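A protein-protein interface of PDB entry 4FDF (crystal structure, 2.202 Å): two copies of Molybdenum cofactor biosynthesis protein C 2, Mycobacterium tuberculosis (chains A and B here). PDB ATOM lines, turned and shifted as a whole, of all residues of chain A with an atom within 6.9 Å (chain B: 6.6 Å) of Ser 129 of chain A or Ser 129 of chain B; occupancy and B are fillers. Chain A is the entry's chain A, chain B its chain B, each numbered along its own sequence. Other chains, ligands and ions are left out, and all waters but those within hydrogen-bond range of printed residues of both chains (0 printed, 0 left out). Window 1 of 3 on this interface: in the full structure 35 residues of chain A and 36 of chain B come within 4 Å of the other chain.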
ATOM      1  N   ALA A  42      -2.261 -28.702   5.081  1.00  0.00           N
ATOM      2  CA  ALA A  42      -3.187 -29.025   6.163  1.00  0.00           C
ATOM      3  C   ALA A  42      -2.430 -29.262   7.469  1.00  0.00           C
ATOM      4  O   ALA A  42      -1.193 -29.251   7.495  1.00  0.00           O
ATOM      5  CB  ALA A  42      -4.051 -30.256   5.804  1.00  0.00           C
ATOM      6  N   GLY A  73      -4.689 -16.924  10.372  1.00  0.00           N
ATOM      7  CA  GLY A  73      -4.053 -17.698   9.316  1.00  0.00           C
ATOM      8  C   GLY A  73      -4.001 -16.973   7.982  1.00  0.00           C
ATOM      9  O   GLY A  73      -2.975 -16.987   7.306  1.00  0.00           O
ATOM     10  N   ALA A  76      -1.401 -14.446   8.341  1.00  0.00           N
ATOM     11  CA  ALA A  76      -0.087 -15.088   8.449  1.00  0.00           C
ATOM     12  C   ALA A  76       0.462 -15.499   7.090  1.00  0.00           C
ATOM     13  O   ALA A  76       1.676 -15.435   6.863  1.00  0.00           O
ATOM     14  CB  ALA A  76      -0.142 -16.284   9.372  1.00  0.00           C
ATOM     15  N   ILE A 108      -7.201 -28.399   9.735  1.00  0.00           N
ATOM     16  CA  ILE A 108      -7.141 -27.084   9.116  1.00  0.00           C
ATOM     17  C   ILE A 108      -6.523 -27.249   7.745  1.00  0.00           C
ATOM     18  O   ILE A 108      -5.449 -27.840   7.603  1.00  0.00           O
ATOM     19  CB  ILE A 108      -6.303 -26.101   9.957  1.00  0.00           C
ATOM     20  CG1 ILE A 108      -6.866 -26.017  11.384  1.00  0.00           C
ATOM     21  CG2 ILE A 108      -6.286 -24.718   9.308  1.00  0.00           C
ATOM     22  CD1 ILE A 108      -5.815 -25.894  12.470  1.00  0.00           C
ATOM     23  N   ALA A 124       1.037 -21.378   2.506  1.00  0.00           N
ATOM     24  CA  ALA A 124       0.016 -22.335   2.960  1.00  0.00           C
ATOM     25  C   ALA A 124       0.354 -22.966   4.314  1.00  0.00           C
ATOM     26  O   ALA A 124      -0.479 -23.012   5.221  1.00  0.00           O
ATOM     27  CB  ALA A 124      -0.220 -23.424   1.893  1.00  0.00           C
ATOM     28  N   LEU A 125       1.585 -23.443   4.443  1.00  0.00           N
ATOM     29  CA  LEU A 125       2.038 -24.023   5.697  1.00  0.00           C
ATOM     30  C   LEU A 125       1.948 -23.041   6.873  1.00  0.00           C
ATOM     31  O   LEU A 125       1.545 -23.432   7.966  1.00  0.00           O
ATOM     32  CB  LEU A 125       3.472 -24.541   5.549  1.00  0.00           C
ATOM     33  CG  LEU A 125       3.674 -25.786   4.688  1.00  0.00           C
ATOM     34  CD1 LEU A 125       5.131 -25.893   4.346  1.00  0.00           C
ATOM     35  CD2 LEU A 125       3.162 -27.064   5.387  1.00  0.00           C
ATOM     36  N   THR A 126       2.314 -21.773   6.650  1.00  0.00           N
ATOM     37  CA  THR A 126       2.312 -20.794   7.740  1.00  0.00           C
ATOM     38  C   THR A 126       0.900 -20.410   8.123  1.00  0.00           C
ATOM     39  O   THR A 126       0.603 -20.179   9.303  1.00  0.00           O
ATOM     40  CB  THR A 126       3.132 -19.515   7.429  1.00  0.00           C
ATOM     41  OG1 THR A 126       2.372 -18.652   6.579  1.00  0.00           O
ATOM     42  CG2 THR A 126       4.464 -19.848   6.765  1.00  0.00           C
ATOM     43  N   ALA A 127       0.023 -20.334   7.125  1.00  0.00           N
ATOM     44  CA  ALA A 127      -1.382 -20.152   7.393  1.00  0.00           C
ATOM     45  C   ALA A 127      -1.900 -21.279   8.309  1.00  0.00           C
ATOM     46  O   ALA A 127      -2.505 -21.016   9.350  1.00  0.00           O
ATOM     47  CB  ALA A 127      -2.163 -20.082   6.078  1.00  0.00           C
ATOM     48  N   VAL A 128      -1.630 -22.525   7.935  1.00  0.00           N
ATOM     49  CA  VAL A 128      -2.008 -23.680   8.753  1.00  0.00           C
ATOM     50  C   VAL A 128      -1.464 -23.530  10.184  1.00  0.00           C
ATOM     51  O   VAL A 128      -2.224 -23.632  11.167  1.00  0.00           O
ATOM     52  CB  VAL A 128      -1.532 -25.033   8.111  1.00  0.00           C
ATOM     53  CG1 VAL A 128      -1.562 -26.169   9.139  1.00  0.00           C
ATOM     54  CG2 VAL A 128      -2.404 -25.393   6.918  1.00  0.00           C
ATOM     55  N   SER A 129      -0.163 -23.256  10.293  1.00  0.00           N
ATOM     56  CA  SER A 129       0.510 -23.185  11.596  1.00  0.00           C
ATOM     57  C   SER A 129      -0.069 -22.123  12.536  1.00  0.00           C
ATOM     58  O   SER A 129      -0.279 -22.380  13.731  1.00  0.00           O
ATOM     59  CB  SER A 129       2.005 -22.963  11.401  1.00  0.00           C
ATOM     60  OG  SER A 129       2.530 -23.937  10.518  1.00  0.00           O
ATOM     61  N   VAL A 130      -0.373 -20.956  11.982  1.00  0.00           N
ATOM     62  CA  VAL A 130      -0.833 -19.820  12.789  1.00  0.00           C
ATOM     63  C   VAL A 130      -2.325 -19.911  13.145  1.00  0.00           C
ATOM     64  O   VAL A 130      -2.746 -19.508  14.233  1.00  0.00           O
ATOM     65  CB  VAL A 130      -0.441 -18.475  12.116  1.00  0.00           C
ATOM     66  CG1 VAL A 130      -1.014 -17.271  12.880  1.00  0.00           C
ATOM     67  CG2 VAL A 130       1.096 -18.360  12.037  1.00  0.00           C
ATOM     68  N   ALA A 131      -3.121 -20.462  12.235  1.00  0.00           N
ATOM     69  CA  ALA A 131      -4.487 -20.841  12.577  1.00  0.00           C
ATOM     70  C   ALA A 131      -4.461 -21.814  13.770  1.00  0.00           C
ATOM     71  O   ALA A 131      -5.245 -21.673  14.711  1.00  0.00           O
ATOM     72  CB  ALA A 131      -5.196 -21.476  11.363  1.00  0.00           C
ATOM     73  N   ALA A 132      -3.542 -22.785  13.735  1.00  0.00           N
ATOM     74  CA  ALA A 132      -3.491 -23.832  14.768  1.00  0.00           C
ATOM     75  C   ALA A 132      -3.020 -23.258  16.083  1.00  0.00           C
ATOM     76  O   ALA A 132      -3.538 -23.612  17.140  1.00  0.00           O
ATOM     77  CB  ALA A 132      -2.584 -25.018  14.333  1.00  0.00           C
ATOM     78  N   LEU A 133      -2.049 -22.342  16.012  1.00  0.00           N
ATOM     79  CA  LEU A 133      -1.560 -21.681  17.202  1.00  0.00           C
ATOM     80  C   LEU A 133      -2.669 -20.847  17.825  1.00  0.00           C
ATOM     81  O   LEU A 133      -2.810 -20.814  19.051  1.00  0.00           O
ATOM     82  CB  LEU A 133      -0.331 -20.823  16.896  1.00  0.00           C
ATOM     83  CG  LEU A 133       1.006 -21.550  16.675  1.00  0.00           C
ATOM     84  CD1 LEU A 133       1.980 -20.594  16.027  1.00  0.00           C
ATOM     85  CD2 LEU A 133       1.621 -22.150  17.946  1.00  0.00           C
ATOM     86  N   THR A 134      -3.449 -20.182  16.972  1.00  0.00           N
ATOM     87  CA  THR A 134      -4.571 -19.379  17.420  1.00  0.00           C
ATOM     88  C   THR A 134      -5.661 -20.221  18.066  1.00  0.00           C
ATOM     89  O   THR A 134      -6.100 -19.915  19.180  1.00  0.00           O
ATOM     90  CB  THR A 134      -5.161 -18.506  16.273  1.00  0.00           C
ATOM     91  OG1 THR A 134      -4.114 -17.712  15.708  1.00  0.00           O
ATOM     92  CG2 THR A 134      -6.233 -17.577  16.817  1.00  0.00           C
ATOM     93  N   ILE A 148      -0.629 -29.849  18.305  1.00  0.00           N
ATOM     94  CA  ILE A 148      -0.679 -29.446  16.894  1.00  0.00           C
ATOM     95  C   ILE A 148       0.159 -30.447  16.094  1.00  0.00           C
ATOM     96  O   ILE A 148       1.371 -30.583  16.301  1.00  0.00           O
ATOM     97  CB  ILE A 148      -0.178 -27.974  16.660  1.00  0.00           C
ATOM     98  CG1 ILE A 148      -1.092 -26.966  17.365  1.00  0.00           C
ATOM     99  CG2 ILE A 148      -0.125 -27.648  15.184  1.00  0.00           C
ATOM    100  CD1 ILE A 148      -0.496 -25.553  17.534  1.00  0.00           C
ATOM    101  N   ILE A 151       1.395 -31.202  10.277  1.00  0.00           N
ATOM    102  CA  ILE A 151       1.468 -30.074   9.359  1.00  0.00           C
ATOM    103  C   ILE A 151       2.270 -30.485   8.111  1.00  0.00           C
ATOM    104  O   ILE A 151       3.440 -30.874   8.206  1.00  0.00           O
ATOM    105  CB  ILE A 151       2.045 -28.790  10.057  1.00  0.00           C
ATOM    106  CG1 ILE A 151       1.078 -28.288  11.135  1.00  0.00           C
ATOM    107  CG2 ILE A 151       2.315 -27.663   9.037  1.00  0.00           C
ATOM    108  CD1 ILE A 151       1.640 -27.165  12.008  1.00  0.00           C
ATOM    109  N   ILE B  84      -0.875 -13.717  16.800  1.00  0.00           N
ATOM    110  CA  ILE B  84      -1.997 -14.345  17.497  1.00  0.00           C
ATOM    111  C   ILE B  84      -2.876 -13.255  18.103  1.00  0.00           C
ATOM    112  O   ILE B  84      -2.497 -12.620  19.084  1.00  0.00           O
ATOM    113  CB  ILE B  84      -1.525 -15.302  18.626  1.00  0.00           C
ATOM    114  CG1 ILE B  84      -0.399 -16.235  18.140  1.00  0.00           C
ATOM    115  CG2 ILE B  84      -2.713 -16.069  19.211  1.00  0.00           C
ATOM    116  CD1 ILE B  84      -0.806 -17.223  17.020  1.00  0.00           C
ATOM    117  N   ILE B 108      12.820 -29.963  18.150  1.00  0.00           N
ATOM    118  CA  ILE B 108      13.011 -28.554  18.416  1.00  0.00           C
ATOM    119  C   ILE B 108      12.489 -28.261  19.820  1.00  0.00           C
ATOM    120  O   ILE B 108      11.408 -28.696  20.189  1.00  0.00           O
ATOM    121  CB  ILE B 108      12.266 -27.690  17.366  1.00  0.00           C
ATOM    122  CG1 ILE B 108      12.645 -28.127  15.951  1.00  0.00           C
ATOM    123  CG2 ILE B 108      12.569 -26.208  17.563  1.00  0.00           C
ATOM    124  CD1 ILE B 108      11.650 -27.744  14.887  1.00  0.00           C
ATOM    125  N   ALA B 124       6.651 -19.601  23.327  1.00  0.00           N
ATOM    126  CA  ALA B 124       7.399 -20.843  23.199  1.00  0.00           C
ATOM    127  C   ALA B 124       6.895 -21.693  22.023  1.00  0.00           C
ATOM    128  O   ALA B 124       7.702 -22.186  21.223  1.00  0.00           O
ATOM    129  CB  ALA B 124       7.363 -21.644  24.505  1.00  0.00           C
ATOM    130  N   LEU B 125       5.576 -21.856  21.921  1.00  0.00           N
ATOM    131  CA  LEU B 125       4.960 -22.609  20.816  1.00  0.00           C
ATOM    132  C   LEU B 125       5.182 -21.953  19.443  1.00  0.00           C
ATOM    133  O   LEU B 125       5.416 -22.644  18.444  1.00  0.00           O
ATOM    134  CB  LEU B 125       3.461 -22.783  21.063  1.00  0.00           C
ATOM    135  CG  LEU B 125       3.048 -23.715  22.197  1.00  0.00           C
ATOM    136  CD1 LEU B 125       1.598 -23.425  22.586  1.00  0.00           C
ATOM    137  CD2 LEU B 125       3.234 -25.187  21.834  1.00  0.00           C
ATOM    138  N   THR B 126       5.109 -20.626  19.407  1.00  0.00           N
ATOM    139  CA  THR B 126       5.319 -19.841  18.188  1.00  0.00           C
ATOM    140  C   THR B 126       6.760 -19.991  17.657  1.00  0.00           C
ATOM    141  O   THR B 126       6.982 -20.200  16.449  1.00  0.00           O
ATOM    142  CB  THR B 126       4.935 -18.358  18.450  1.00  0.00           C
ATOM    143  OG1 THR B 126       3.529 -18.284  18.742  1.00  0.00           O
ATOM    144  CG2 THR B 126       5.241 -17.471  17.272  1.00  0.00           C
ATOM    145  N   ALA B 127       7.726 -19.900  18.572  1.00  0.00           N
ATOM    146  CA  ALA B 127       9.143 -20.113  18.274  1.00  0.00           C
ATOM    147  C   ALA B 127       9.395 -21.506  17.706  1.00  0.00           C
ATOM    148  O   ALA B 127      10.017 -21.656  16.661  1.00  0.00           O
ATOM    149  CB  ALA B 127       9.987 -19.890  19.537  1.00  0.00           C
ATOM    150  N   VAL B 128       8.878 -22.527  18.379  1.00  0.00           N
ATOM    151  CA  VAL B 128       9.001 -23.898  17.897  1.00  0.00           C
ATOM    152  C   VAL B 128       8.384 -23.976  16.508  1.00  0.00           C
ATOM    153  O   VAL B 128       8.955 -24.529  15.568  1.00  0.00           O
ATOM    154  CB  VAL B 128       8.292 -24.888  18.855  1.00  0.00           C
ATOM    155  CG1 VAL B 128       7.985 -26.231  18.155  1.00  0.00           C
ATOM    156  CG2 VAL B 128       9.131 -25.119  20.104  1.00  0.00           C
ATOM    157  N   SER B 129       7.225 -23.360  16.383  1.00  0.00           N
ATOM    158  CA  SER B 129       6.476 -23.398  15.160  1.00  0.00           C
ATOM    159  C   SER B 129       7.207 -22.739  14.008  1.00  0.00           C
ATOM    160  O   SER B 129       7.344 -23.343  12.931  1.00  0.00           O
ATOM    161  CB  SER B 129       5.145 -22.726  15.408  1.00  0.00           C
ATOM    162  OG  SER B 129       4.296 -22.933  14.296  1.00  0.00           O
ATOM    163  N   VAL B 130       7.711 -21.520  14.220  1.00  0.00           N
ATOM    164  CA  VAL B 130       8.397 -20.815  13.132  1.00  0.00           C
ATOM    165  C   VAL B 130       9.767 -21.436  12.818  1.00  0.00           C
ATOM    166  O   VAL B 130      10.200 -21.443  11.660  1.00  0.00           O
ATOM    167  CB  VAL B 130       8.456 -19.278  13.364  1.00  0.00           C
ATOM    168  CG1 VAL B 130       9.316 -18.588  12.302  1.00  0.00           C
ATOM    169  CG2 VAL B 130       7.022 -18.684  13.338  1.00  0.00           C
ATOM    170  N   ALA B 131      10.433 -21.976  13.835  1.00  0.00           N
ATOM    171  CA  ALA B 131      11.698 -22.694  13.636  1.00  0.00           C
ATOM    172  C   ALA B 131      11.508 -23.940  12.773  1.00  0.00           C
ATOM    173  O   ALA B 131      12.369 -24.255  11.950  1.00  0.00           O
ATOM    174  CB  ALA B 131      12.326 -23.067  14.983  1.00  0.00           C
ATOM    175  N   ALA B 132      10.389 -24.641  12.970  1.00  0.00           N
ATOM    176  CA  ALA B 132      10.037 -25.823  12.174  1.00  0.00           C
ATOM    177  C   ALA B 132       9.730 -25.439  10.736  1.00  0.00           C
ATOM    178  O   ALA B 132      10.219 -26.071   9.805  1.00  0.00           O
ATOM    179  CB  ALA B 132       8.831 -26.541  12.783  1.00  0.00           C
ATOM    180  N   LEU B 133       8.921 -24.399  10.557  1.00  0.00           N
ATOM    181  CA  LEU B 133       8.647 -23.879   9.222  1.00  0.00           C
ATOM    182  C   LEU B 133       9.929 -23.474   8.495  1.00  0.00           C
ATOM    183  O   LEU B 133      10.062 -23.688   7.291  1.00  0.00           O
ATOM    184  CB  LEU B 133       7.683 -22.681   9.276  1.00  0.00           C
ATOM    185  CG  LEU B 133       6.209 -22.951   9.628  1.00  0.00           C
ATOM    186  CD1 LEU B 133       5.493 -21.662  10.035  1.00  0.00           C
ATOM    187  CD2 LEU B 133       5.491 -23.610   8.466  1.00  0.00           C
ATOM    188  N   THR B 134      10.860 -22.880   9.237  1.00  0.00           N
ATOM    189  CA  THR B 134      12.117 -22.433   8.671  1.00  0.00           C
ATOM    190  C   THR B 134      13.014 -23.621   8.333  1.00  0.00           C
ATOM    191  O   THR B 134      13.674 -23.617   7.291  1.00  0.00           O
ATOM    192  CB  THR B 134      12.825 -21.442   9.602  1.00  0.00           C
ATOM    193  OG1 THR B 134      11.991 -20.287   9.752  1.00  0.00           O
ATOM    194  CG2 THR B 134      14.174 -21.023   9.027  1.00  0.00           C
ATOM    195  N   ILE B 148       5.666 -31.596   9.836  1.00  0.00           N
ATOM    196  CA  ILE B 148       5.874 -30.971  11.134  1.00  0.00           C
ATOM    197  C   ILE B 148       4.870 -31.572  12.118  1.00  0.00           C
ATOM    198  O   ILE B 148       3.657 -31.536  11.895  1.00  0.00           O
ATOM    199  CB  ILE B 148       5.734 -29.426  11.043  1.00  0.00           C
ATOM    200  CG1 ILE B 148       6.861 -28.830  10.178  1.00  0.00           C
ATOM    201  CG2 ILE B 148       5.735 -28.797  12.434  1.00  0.00           C
ATOM    202  CD1 ILE B 148       6.594 -27.395   9.683  1.00  0.00           C
ATOM    203  N   ILE B 151       3.796 -30.562  17.991  1.00  0.00           N
ATOM    204  CA  ILE B 151       4.033 -29.271  18.623  1.00  0.00           C
ATOM    205  C   ILE B 151       3.187 -29.169  19.891  1.00  0.00           C
ATOM    206  O   ILE B 151       1.968 -29.238  19.833  1.00  0.00           O
ATOM    207  CB  ILE B 151       3.737 -28.101  17.657  1.00  0.00           C
ATOM    208  CG1 ILE B 151       4.771 -28.111  16.526  1.00  0.00           C
ATOM    209  CG2 ILE B 151       3.720 -26.750  18.424  1.00  0.00           C
ATOM    210  CD1 ILE B 151       4.381 -27.300  15.305  1.00  0.00           C
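O of Ile 148 of chain A is in hydrogen-bond range of N of Ile 151 of chain B (3.0 Å). The backbone NH (N) of Ile 151 of chain A lies within hydrogen-bond range of the backbone carbonyl oxygen (O) of Ile 148 of chain B (2.8 Å).
O of Leu 125 of chain A sits at hydrogen-bond distance from OG of Ser 129 of chain A (2.8 Å). The backbone carbonyl oxygen (O) of Ala 76 of chain A lies within hydrogen-bond range of the side-chain hydroxyl (OG1) of Thr 126 of chain A. OG1 of Thr 134 of chain A sits at hydrogen-bond distance from O of Val 130 of chain A, 2.7 Å away.
CB of Leu 125 of chain A touches CD2 of Leu 133 of chain B, at 3.7 Å. Thr 126 of chain A touches Leu 133 of chain B. Ser 129 of chain A touches Ser 129 of chain B (CB to OG, 3.7 Å). Ser 129 of chain A touches Leu 133 of chain B. Ile 84 of chain B touches Leu 133 of chain A. Leu 133 of chain A touches Leu 125 of chain B (CD2 to CB, 3.7 Å). Leu 133 of chain A touches Thr 126 of chain B (CD1 to OG1, 3.9 Å). Leu 133 of chain A touches Ser 129 of chain B (CD1 to OG, 3.7 Å). OG1 of Thr 134 of chain A touches CD1 of Ile 84 of chain B, at 3.6 Å.
Ser 129 of chain A touches two residues of chain B. Printed residues of chain A within 4 Å of Ile 84 of chain B: Leu 133 (3.6 Å) and Thr 134 (3.6 Å). Of chain A, only Ser 129 and Leu 133 come within 4 Å of Ser 129 of chain B. Printed residues of chain A within 4 Å of Leu 133 of chain B: Leu 125, Thr 126 and Ser 129. Of the printed residues of chain A, Ile 151 of chain B touches Ile 148. The nearest printed residue of chain B that does not touch Ile 151 of chain A is Ile 151 of chain B (4.3 Å).
Of the 15 printed residues of chain B, 7 touch a printed residue of chain A. Hydrophobic or aromatic side chains of chain B that line the printed part of chain A: Ile 84, Leu 125, Leu 133, Ile 148 and Ile 151. Hydrophobic or aromatic side chains of chain A within 4 Å of the printed part of chain B: Leu 125, Leu 133 and Ile 151. Among the printed residues, 11 pairs touch across the chains. Among the printed residues, no Asp or Glu carboxylate lies within 4 Å of a Lys or Arg side-chain nitrogen of the other chain.
Leu 125 of chain A touches Leu 133 of chain B, and with the chains exchanged Leu 133 of chain A touches Leu 125 of chain B. Thr 126 of chain A touches Leu 133 of chain B, and with the chains exchanged Leu 133 of chain A touches Thr 126 of chain B. Ser 129 of chain B touches its own counterpart, Ser 129 of chain A. Ser 129 of chain A touches Leu 133 of chain B, and with the chains exchanged Leu 133 of chain A touches Ser 129 of chain B. 14 positions are printed for both chains.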
